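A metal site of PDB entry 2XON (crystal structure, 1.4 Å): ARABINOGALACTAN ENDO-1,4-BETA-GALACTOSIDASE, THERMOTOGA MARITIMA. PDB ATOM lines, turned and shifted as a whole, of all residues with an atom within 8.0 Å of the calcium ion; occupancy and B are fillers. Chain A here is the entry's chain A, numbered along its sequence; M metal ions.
OE1 of Glu 17 lies within hydrogen-bond range of N of Glu 48. The backbone NH of Glu 17 sits at hydrogen-bond distance from the side-chain amide oxygen of Asn 13 (3.2 Å). The backbone NH (N) of His 45 sits close to the side-chain carboxylate (OD1) of Asp 144 (2.9 Å).
Of the 23 residues printed, 5 come within 4 Å of the calcium ion.
The calcium ion is bound by OE1 of Gln 46. OE2 of Glu 17 is bound to the calcium ion (2.3 Å). The calcium ion is bound by O of Tyr 49 (2.3 Å). The backbone carbonyl oxygen (O) of Gly 15 binds the calcium ion, 2.4 Å away. O of Gln 46 binds the calcium ion, 2.4 Å away. OD2 of Asp 144 binds the calcium ion. The side-chain carboxylate (OD1) of Asp 144 binds the calcium ion, at 2.7 Å. The calcium ion has seven donor atoms within binding distance.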
ATOM      1  N   ASN A  13      14.400 -13.551  22.215  1.00  0.00           N
ATOM      2  CA  ASN A  13      15.504 -12.548  22.092  1.00  0.00           C
ATOM      3  C   ASN A  13      14.969 -11.120  22.068  1.00  0.00           C
ATOM      4  O   ASN A  13      15.345 -10.350  21.185  1.00  0.00           O
ATOM      5  CB  ASN A  13      16.391 -12.879  20.865  1.00  0.00           C
ATOM      6  CG  ASN A  13      17.692 -12.142  20.847  1.00  0.00           C
ATOM      7  OD1 ASN A  13      18.226 -11.746  21.894  1.00  0.00           O
ATOM      8  ND2 ASN A  13      18.229 -11.957  19.618  1.00  0.00           N
ATOM      9  N   PRO A  14      14.157 -10.774  23.067  1.00  0.00           N
ATOM     10  CA  PRO A  14      13.436  -9.472  22.966  1.00  0.00           C
ATOM     11  C   PRO A  14      14.322  -8.270  23.177  1.00  0.00           C
ATOM     12  O   PRO A  14      13.931  -7.147  22.832  1.00  0.00           O
ATOM     13  CB  PRO A  14      12.410  -9.629  24.074  1.00  0.00           C
ATOM     14  CG  PRO A  14      13.105 -10.445  25.120  1.00  0.00           C
ATOM     15  CD  PRO A  14      13.745 -11.525  24.276  1.00  0.00           C
ATOM     16  N   GLY A  15      15.540  -8.468  23.744  1.00  0.00           N
ATOM     17  CA  GLY A  15      16.482  -7.419  24.009  1.00  0.00           C
ATOM     18  C   GLY A  15      17.744  -7.522  23.234  1.00  0.00           C
ATOM     19  O   GLY A  15      18.684  -6.785  23.492  1.00  0.00           O
ATOM     20  N   PHE A  16      17.801  -8.437  22.260  1.00  0.00           N
ATOM     21  CA  PHE A  16      18.992  -8.637  21.404  1.00  0.00           C
ATOM     22  C   PHE A  16      20.248  -9.009  22.194  1.00  0.00           C
ATOM     23  O   PHE A  16      21.353  -8.822  21.717  1.00  0.00           O
ATOM     24  CB  PHE A  16      19.191  -7.419  20.477  1.00  0.00           C
ATOM     25  CG  PHE A  16      17.981  -7.104  19.722  1.00  0.00           C
ATOM     26  CD1 PHE A  16      17.111  -6.106  20.151  1.00  0.00           C
ATOM     27  CD2 PHE A  16      17.626  -7.877  18.611  1.00  0.00           C
ATOM     28  CE1 PHE A  16      15.883  -5.969  19.501  1.00  0.00           C
ATOM     29  CE2 PHE A  16      16.456  -7.683  17.923  1.00  0.00           C
ATOM     30  CZ  PHE A  16      15.566  -6.740  18.395  1.00  0.00           C
ATOM     31  N   GLU A  17      20.053  -9.573  23.398  1.00  0.00           N
ATOM     32  CA  GLU A  17      21.144  -9.832  24.328  1.00  0.00           C
ATOM     33  C   GLU A  17      22.023 -11.005  23.913  1.00  0.00           C
ATOM     34  O   GLU A  17      23.065 -11.206  24.505  1.00  0.00           O
ATOM     35  CB  GLU A  17      20.673  -9.953  25.759  1.00  0.00           C
ATOM     36  CG  GLU A  17      20.106  -8.633  26.291  1.00  0.00           C
ATOM     37  CD  GLU A  17      21.128  -7.473  26.259  1.00  0.00           C
ATOM     38  OE1 GLU A  17      22.238  -7.697  26.814  1.00  0.00           O
ATOM     39  OE2 GLU A  17      20.801  -6.369  25.732  1.00  0.00           O
ATOM     40  N   THR A  18      21.663 -11.749  22.877  1.00  0.00           N
ATOM     41  CA  THR A  18      22.562 -12.666  22.271  1.00  0.00           C
ATOM     42  C   THR A  18      23.624 -12.013  21.427  1.00  0.00           C
ATOM     43  O   THR A  18      24.567 -12.689  20.971  1.00  0.00           O
ATOM     44  CB  THR A  18      21.815 -13.626  21.381  1.00  0.00           C
ATOM     45  OG1 THR A  18      21.236 -12.904  20.326  1.00  0.00           O
ATOM     46  CG2 THR A  18      20.733 -14.446  22.114  1.00  0.00           C
ATOM     47  N   VAL A  35      22.914  -5.548  15.151  1.00  0.00           N
ATOM     48  CA  VAL A  35      22.865  -5.675  16.616  1.00  0.00           C
ATOM     49  C   VAL A  35      24.262  -5.291  17.104  1.00  0.00           C
ATOM     50  O   VAL A  35      25.257  -5.842  16.641  1.00  0.00           O
ATOM     51  CB  VAL A  35      22.457  -7.082  17.030  1.00  0.00           C
ATOM     52  CG1 VAL A  35      22.575  -7.177  18.568  1.00  0.00           C
ATOM     53  CG2 VAL A  35      21.044  -7.426  16.606  1.00  0.00           C
ATOM     54  N   VAL A  36      24.327  -4.366  18.055  1.00  0.00           N
ATOM     55  CA  VAL A  36      25.597  -3.870  18.565  1.00  0.00           C
ATOM     56  C   VAL A  36      25.592  -3.920  20.093  1.00  0.00           C
ATOM     57  O   VAL A  36      24.556  -3.831  20.746  1.00  0.00           O
ATOM     58  CB  VAL A  36      25.867  -2.402  18.110  1.00  0.00           C
ATOM     59  CG1 VAL A  36      25.810  -2.272  16.537  1.00  0.00           C
ATOM     60  CG2 VAL A  36      24.894  -1.403  18.731  1.00  0.00           C
ATOM     61  N   ALA A  38      26.125  -1.706  22.872  1.00  0.00           N
ATOM     62  CA  ALA A  38      25.902  -0.249  22.947  1.00  0.00           C
ATOM     63  C   ALA A  38      27.088   0.429  23.611  1.00  0.00           C
ATOM     64  O   ALA A  38      27.542   0.031  24.661  1.00  0.00           O
ATOM     65  CB  ALA A  38      24.579   0.098  23.673  1.00  0.00           C
ATOM     66  N   SER A  41      26.625   2.537  26.879  1.00  0.00           N
ATOM     67  CA  SER A  41      25.555   1.616  27.193  1.00  0.00           C
ATOM     68  C   SER A  41      24.179   2.249  27.261  1.00  0.00           C
ATOM     69  O   SER A  41      23.187   1.543  27.076  1.00  0.00           O
ATOM     70  CB  SER A  41      25.855   0.808  28.506  1.00  0.00           C
ATOM     71  OG  SER A  41      25.784   1.703  29.626  1.00  0.00           O
ATOM     72  N   ASN A  43      22.773   3.841  25.107  1.00  0.00           N
ATOM     73  CA  ASN A  43      22.032   3.673  23.845  1.00  0.00           C
ATOM     74  C   ASN A  43      21.086   2.470  23.852  1.00  0.00           C
ATOM     75  O   ASN A  43      20.143   2.465  23.082  1.00  0.00           O
ATOM     76  CB  ASN A  43      22.993   3.549  22.639  1.00  0.00           C
ATOM     77  CG  ASN A  43      23.602   4.888  22.295  1.00  0.00           C
ATOM     78  OD1 ASN A  43      22.906   5.915  22.435  1.00  0.00           O
ATOM     79  ND2 ASN A  43      24.852   4.892  21.803  1.00  0.00           N
ATOM     80  N   ALA A  44      21.367   1.490  24.742  1.00  0.00           N
ATOM     81  CA  ALA A  44      20.461   0.386  24.932  1.00  0.00           C
ATOM     82  C   ALA A  44      19.453   0.729  26.032  1.00  0.00           C
ATOM     83  O   ALA A  44      19.748   1.526  26.884  1.00  0.00           O
ATOM     84  CB  ALA A  44      21.228  -0.905  25.346  1.00  0.00           C
ATOM     85  N   HIS A  45      18.271   0.101  25.993  1.00  0.00           N
ATOM     86  CA  HIS A  45      17.304   0.322  27.034  1.00  0.00           C
ATOM     87  C   HIS A  45      17.383  -0.709  28.129  1.00  0.00           C
ATOM     88  O   HIS A  45      16.974  -0.423  29.237  1.00  0.00           O
ATOM     89  CB  HIS A  45      15.868   0.340  26.428  1.00  0.00           C
ATOM     90  CG  HIS A  45      14.875   0.984  27.362  1.00  0.00           C
ATOM     91  ND1 HIS A  45      13.948   0.267  28.114  1.00  0.00           N
ATOM     92  CD2 HIS A  45      14.682   2.302  27.657  1.00  0.00           C
ATOM     93  CE1 HIS A  45      13.259   1.120  28.841  1.00  0.00           C
ATOM     94  NE2 HIS A  45      13.682   2.357  28.582  1.00  0.00           N
ATOM     95  N   GLN A  46      17.870  -1.883  27.836  1.00  0.00           N
ATOM     96  CA  GLN A  46      18.150  -2.924  28.830  1.00  0.00           C
ATOM     97  C   GLN A  46      19.327  -3.686  28.332  1.00  0.00           C
ATOM     98  O   GLN A  46      19.545  -3.828  27.154  1.00  0.00           O
ATOM     99  CB  GLN A  46      16.945  -3.823  29.122  1.00  0.00           C
ATOM    100  CG  GLN A  46      16.417  -4.684  28.020  1.00  0.00           C
ATOM    101  CD  GLN A  46      17.197  -5.957  27.672  1.00  0.00           C
ATOM    102  OE1 GLN A  46      17.724  -6.056  26.568  1.00  0.00           O
ATOM    103  NE2 GLN A  46      17.266  -6.917  28.620  1.00  0.00           N
ATOM    104  N   GLY A  47      20.067  -4.288  29.275  1.00  0.00           N
ATOM    105  CA  GLY A  47      21.199  -5.108  28.945  1.00  0.00           C
ATOM    106  C   GLY A  47      22.275  -4.322  28.267  1.00  0.00           C
ATOM    107  O   GLY A  47      22.424  -3.126  28.512  1.00  0.00           O
ATOM    108  N   GLU A  48      23.061  -5.028  27.474  1.00  0.00           N
ATOM    109  CA  GLU A  48      24.246  -4.448  26.837  1.00  0.00           C
ATOM    110  C   GLU A  48      24.099  -4.226  25.351  1.00  0.00           C
ATOM    111  O   GLU A  48      24.930  -3.536  24.749  1.00  0.00           O
ATOM    112  CB  GLU A  48      25.467  -5.304  27.092  1.00  0.00           C
ATOM    113  CG  GLU A  48      25.773  -5.483  28.586  1.00  0.00           C
ATOM    114  CD  GLU A  48      27.187  -5.899  28.810  1.00  0.00           C
ATOM    115  OE1 GLU A  48      27.506  -7.072  28.594  1.00  0.00           O
ATOM    116  OE2 GLU A  48      28.033  -5.011  29.099  1.00  0.00           O
ATOM    117  N   TYR A  49      23.063  -4.841  24.772  1.00  0.00           N
ATOM    118  CA  TYR A  49      22.915  -4.806  23.318  1.00  0.00           C
ATOM    119  C   TYR A  49      21.636  -4.167  22.846  1.00  0.00           C
ATOM    120  O   TYR A  49      20.638  -4.129  23.573  1.00  0.00           O
ATOM    121  CB  TYR A  49      22.907  -6.291  22.793  1.00  0.00           C
ATOM    122  CG  TYR A  49      24.214  -6.992  22.873  1.00  0.00           C
ATOM    123  CD1 TYR A  49      25.094  -6.981  21.819  1.00  0.00           C
ATOM    124  CD2 TYR A  49      24.597  -7.656  24.015  1.00  0.00           C
ATOM    125  CE1 TYR A  49      26.331  -7.574  21.895  1.00  0.00           C
ATOM    126  CE2 TYR A  49      25.844  -8.228  24.126  1.00  0.00           C
ATOM    127  CZ  TYR A  49      26.744  -8.208  23.084  1.00  0.00           C
ATOM    128  OH  TYR A  49      27.989  -8.838  23.097  1.00  0.00           O
ATOM    129  N   ALA A  50      21.651  -3.640  21.633  1.00  0.00           N
ATOM    130  CA  ALA A  50      20.467  -3.053  21.007  1.00  0.00           C
ATOM    131  C   ALA A  50      20.663  -3.154  19.527  1.00  0.00           C
ATOM    132  O   ALA A  50      21.760  -3.322  19.043  1.00  0.00           O
ATOM    133  CB  ALA A  50      20.273  -1.592  21.449  1.00  0.00           C
ATOM    134  N   VAL A  51      19.531  -3.035  18.815  1.00  0.00           N
ATOM    135  CA  VAL A  51      19.611  -2.832  17.376  1.00  0.00           C
ATOM    136  C   VAL A  51      20.014  -1.385  17.157  1.00  0.00           C
ATOM    137  O   VAL A  51      19.466  -0.469  17.783  1.00  0.00           O
ATOM    138  CB  VAL A  51      18.234  -3.123  16.733  1.00  0.00           C
ATOM    139  CG1 VAL A  51      18.130  -2.576  15.322  1.00  0.00           C
ATOM    140  CG2 VAL A  51      17.999  -4.644  16.645  1.00  0.00           C
ATOM    141  N   ILE A 143      16.871   0.491  18.668  1.00  0.00           N
ATOM    142  CA  ILE A 143      15.651  -0.243  18.974  1.00  0.00           C
ATOM    143  C   ILE A 143      16.028  -1.316  20.021  1.00  0.00           C
ATOM    144  O   ILE A 143      16.998  -2.046  19.834  1.00  0.00           O
ATOM    145  CB  ILE A 143      15.058  -0.864  17.747  1.00  0.00           C
ATOM    146  CG1 ILE A 143      14.477   0.217  16.825  1.00  0.00           C
ATOM    147  CG2 ILE A 143      13.929  -1.922  18.062  1.00  0.00           C
ATOM    148  CD1 ILE A 143      14.154  -0.258  15.374  1.00  0.00           C
ATOM    149  N   ASP A 144      15.206  -1.473  21.059  1.00  0.00           N
ATOM    150  CA  ASP A 144      15.568  -2.474  22.107  1.00  0.00           C
ATOM    151  C   ASP A 144      14.304  -2.777  22.953  1.00  0.00           C
ATOM    152  O   ASP A 144      13.307  -2.040  22.893  1.00  0.00           O
ATOM    153  CB  ASP A 144      16.672  -1.902  22.990  1.00  0.00           C
ATOM    154  CG  ASP A 144      17.391  -2.919  23.868  1.00  0.00           C
ATOM    155  OD1 ASP A 144      18.140  -2.519  24.772  1.00  0.00           O
ATOM    156  OD2 ASP A 144      17.302  -4.126  23.643  1.00  0.00           O
ATOM    157  N   ASP A 145      14.455  -3.841  23.742  1.00  0.00           N
ATOM    158  CA  ASP A 145      13.593  -4.109  24.868  1.00  0.00           C
ATOM    159  C   ASP A 145      12.114  -4.225  24.435  1.00  0.00           C
ATOM    160  O   ASP A 145      11.228  -3.561  24.968  1.00  0.00           O
ATOM    161  CB  ASP A 145      13.792  -2.980  25.913  1.00  0.00           C
ATOM    162  CG  ASP A 145      13.305  -3.318  27.310  1.00  0.00           C
ATOM    163  OD1 ASP A 145      12.948  -4.470  27.587  1.00  0.00           O
ATOM    164  OD2 ASP A 145      13.351  -2.373  28.119  1.00  0.00           O
ATOM    165  N   PHE A 146      11.914  -5.173  23.551  1.00  0.00           N
ATOM    166  CA  PHE A 146      10.575  -5.629  23.186  1.00  0.00           C
ATOM    167  C   PHE A 146       9.904  -6.400  24.305  1.00  0.00           C
ATOM    168  O   PHE A 146      10.561  -7.082  25.080  1.00  0.00           O
ATOM    169  CB  PHE A 146      10.589  -6.545  21.962  1.00  0.00           C
ATOM    170  CG  PHE A 146      10.781  -5.858  20.665  1.00  0.00           C
ATOM    171  CD1 PHE A 146      12.040  -5.608  20.159  1.00  0.00           C
ATOM    172  CD2 PHE A 146       9.690  -5.456  19.916  1.00  0.00           C
ATOM    173  CE1 PHE A 146      12.201  -4.990  18.892  1.00  0.00           C
ATOM    174  CE2 PHE A 146       9.879  -4.825  18.677  1.00  0.00           C
ATOM    175  CZ  PHE A 146      11.152  -4.638  18.190  1.00  0.00           C
HETATM  176 CA    CA M   1      19.089  -4.983  25.065  1.00  0.00          CA
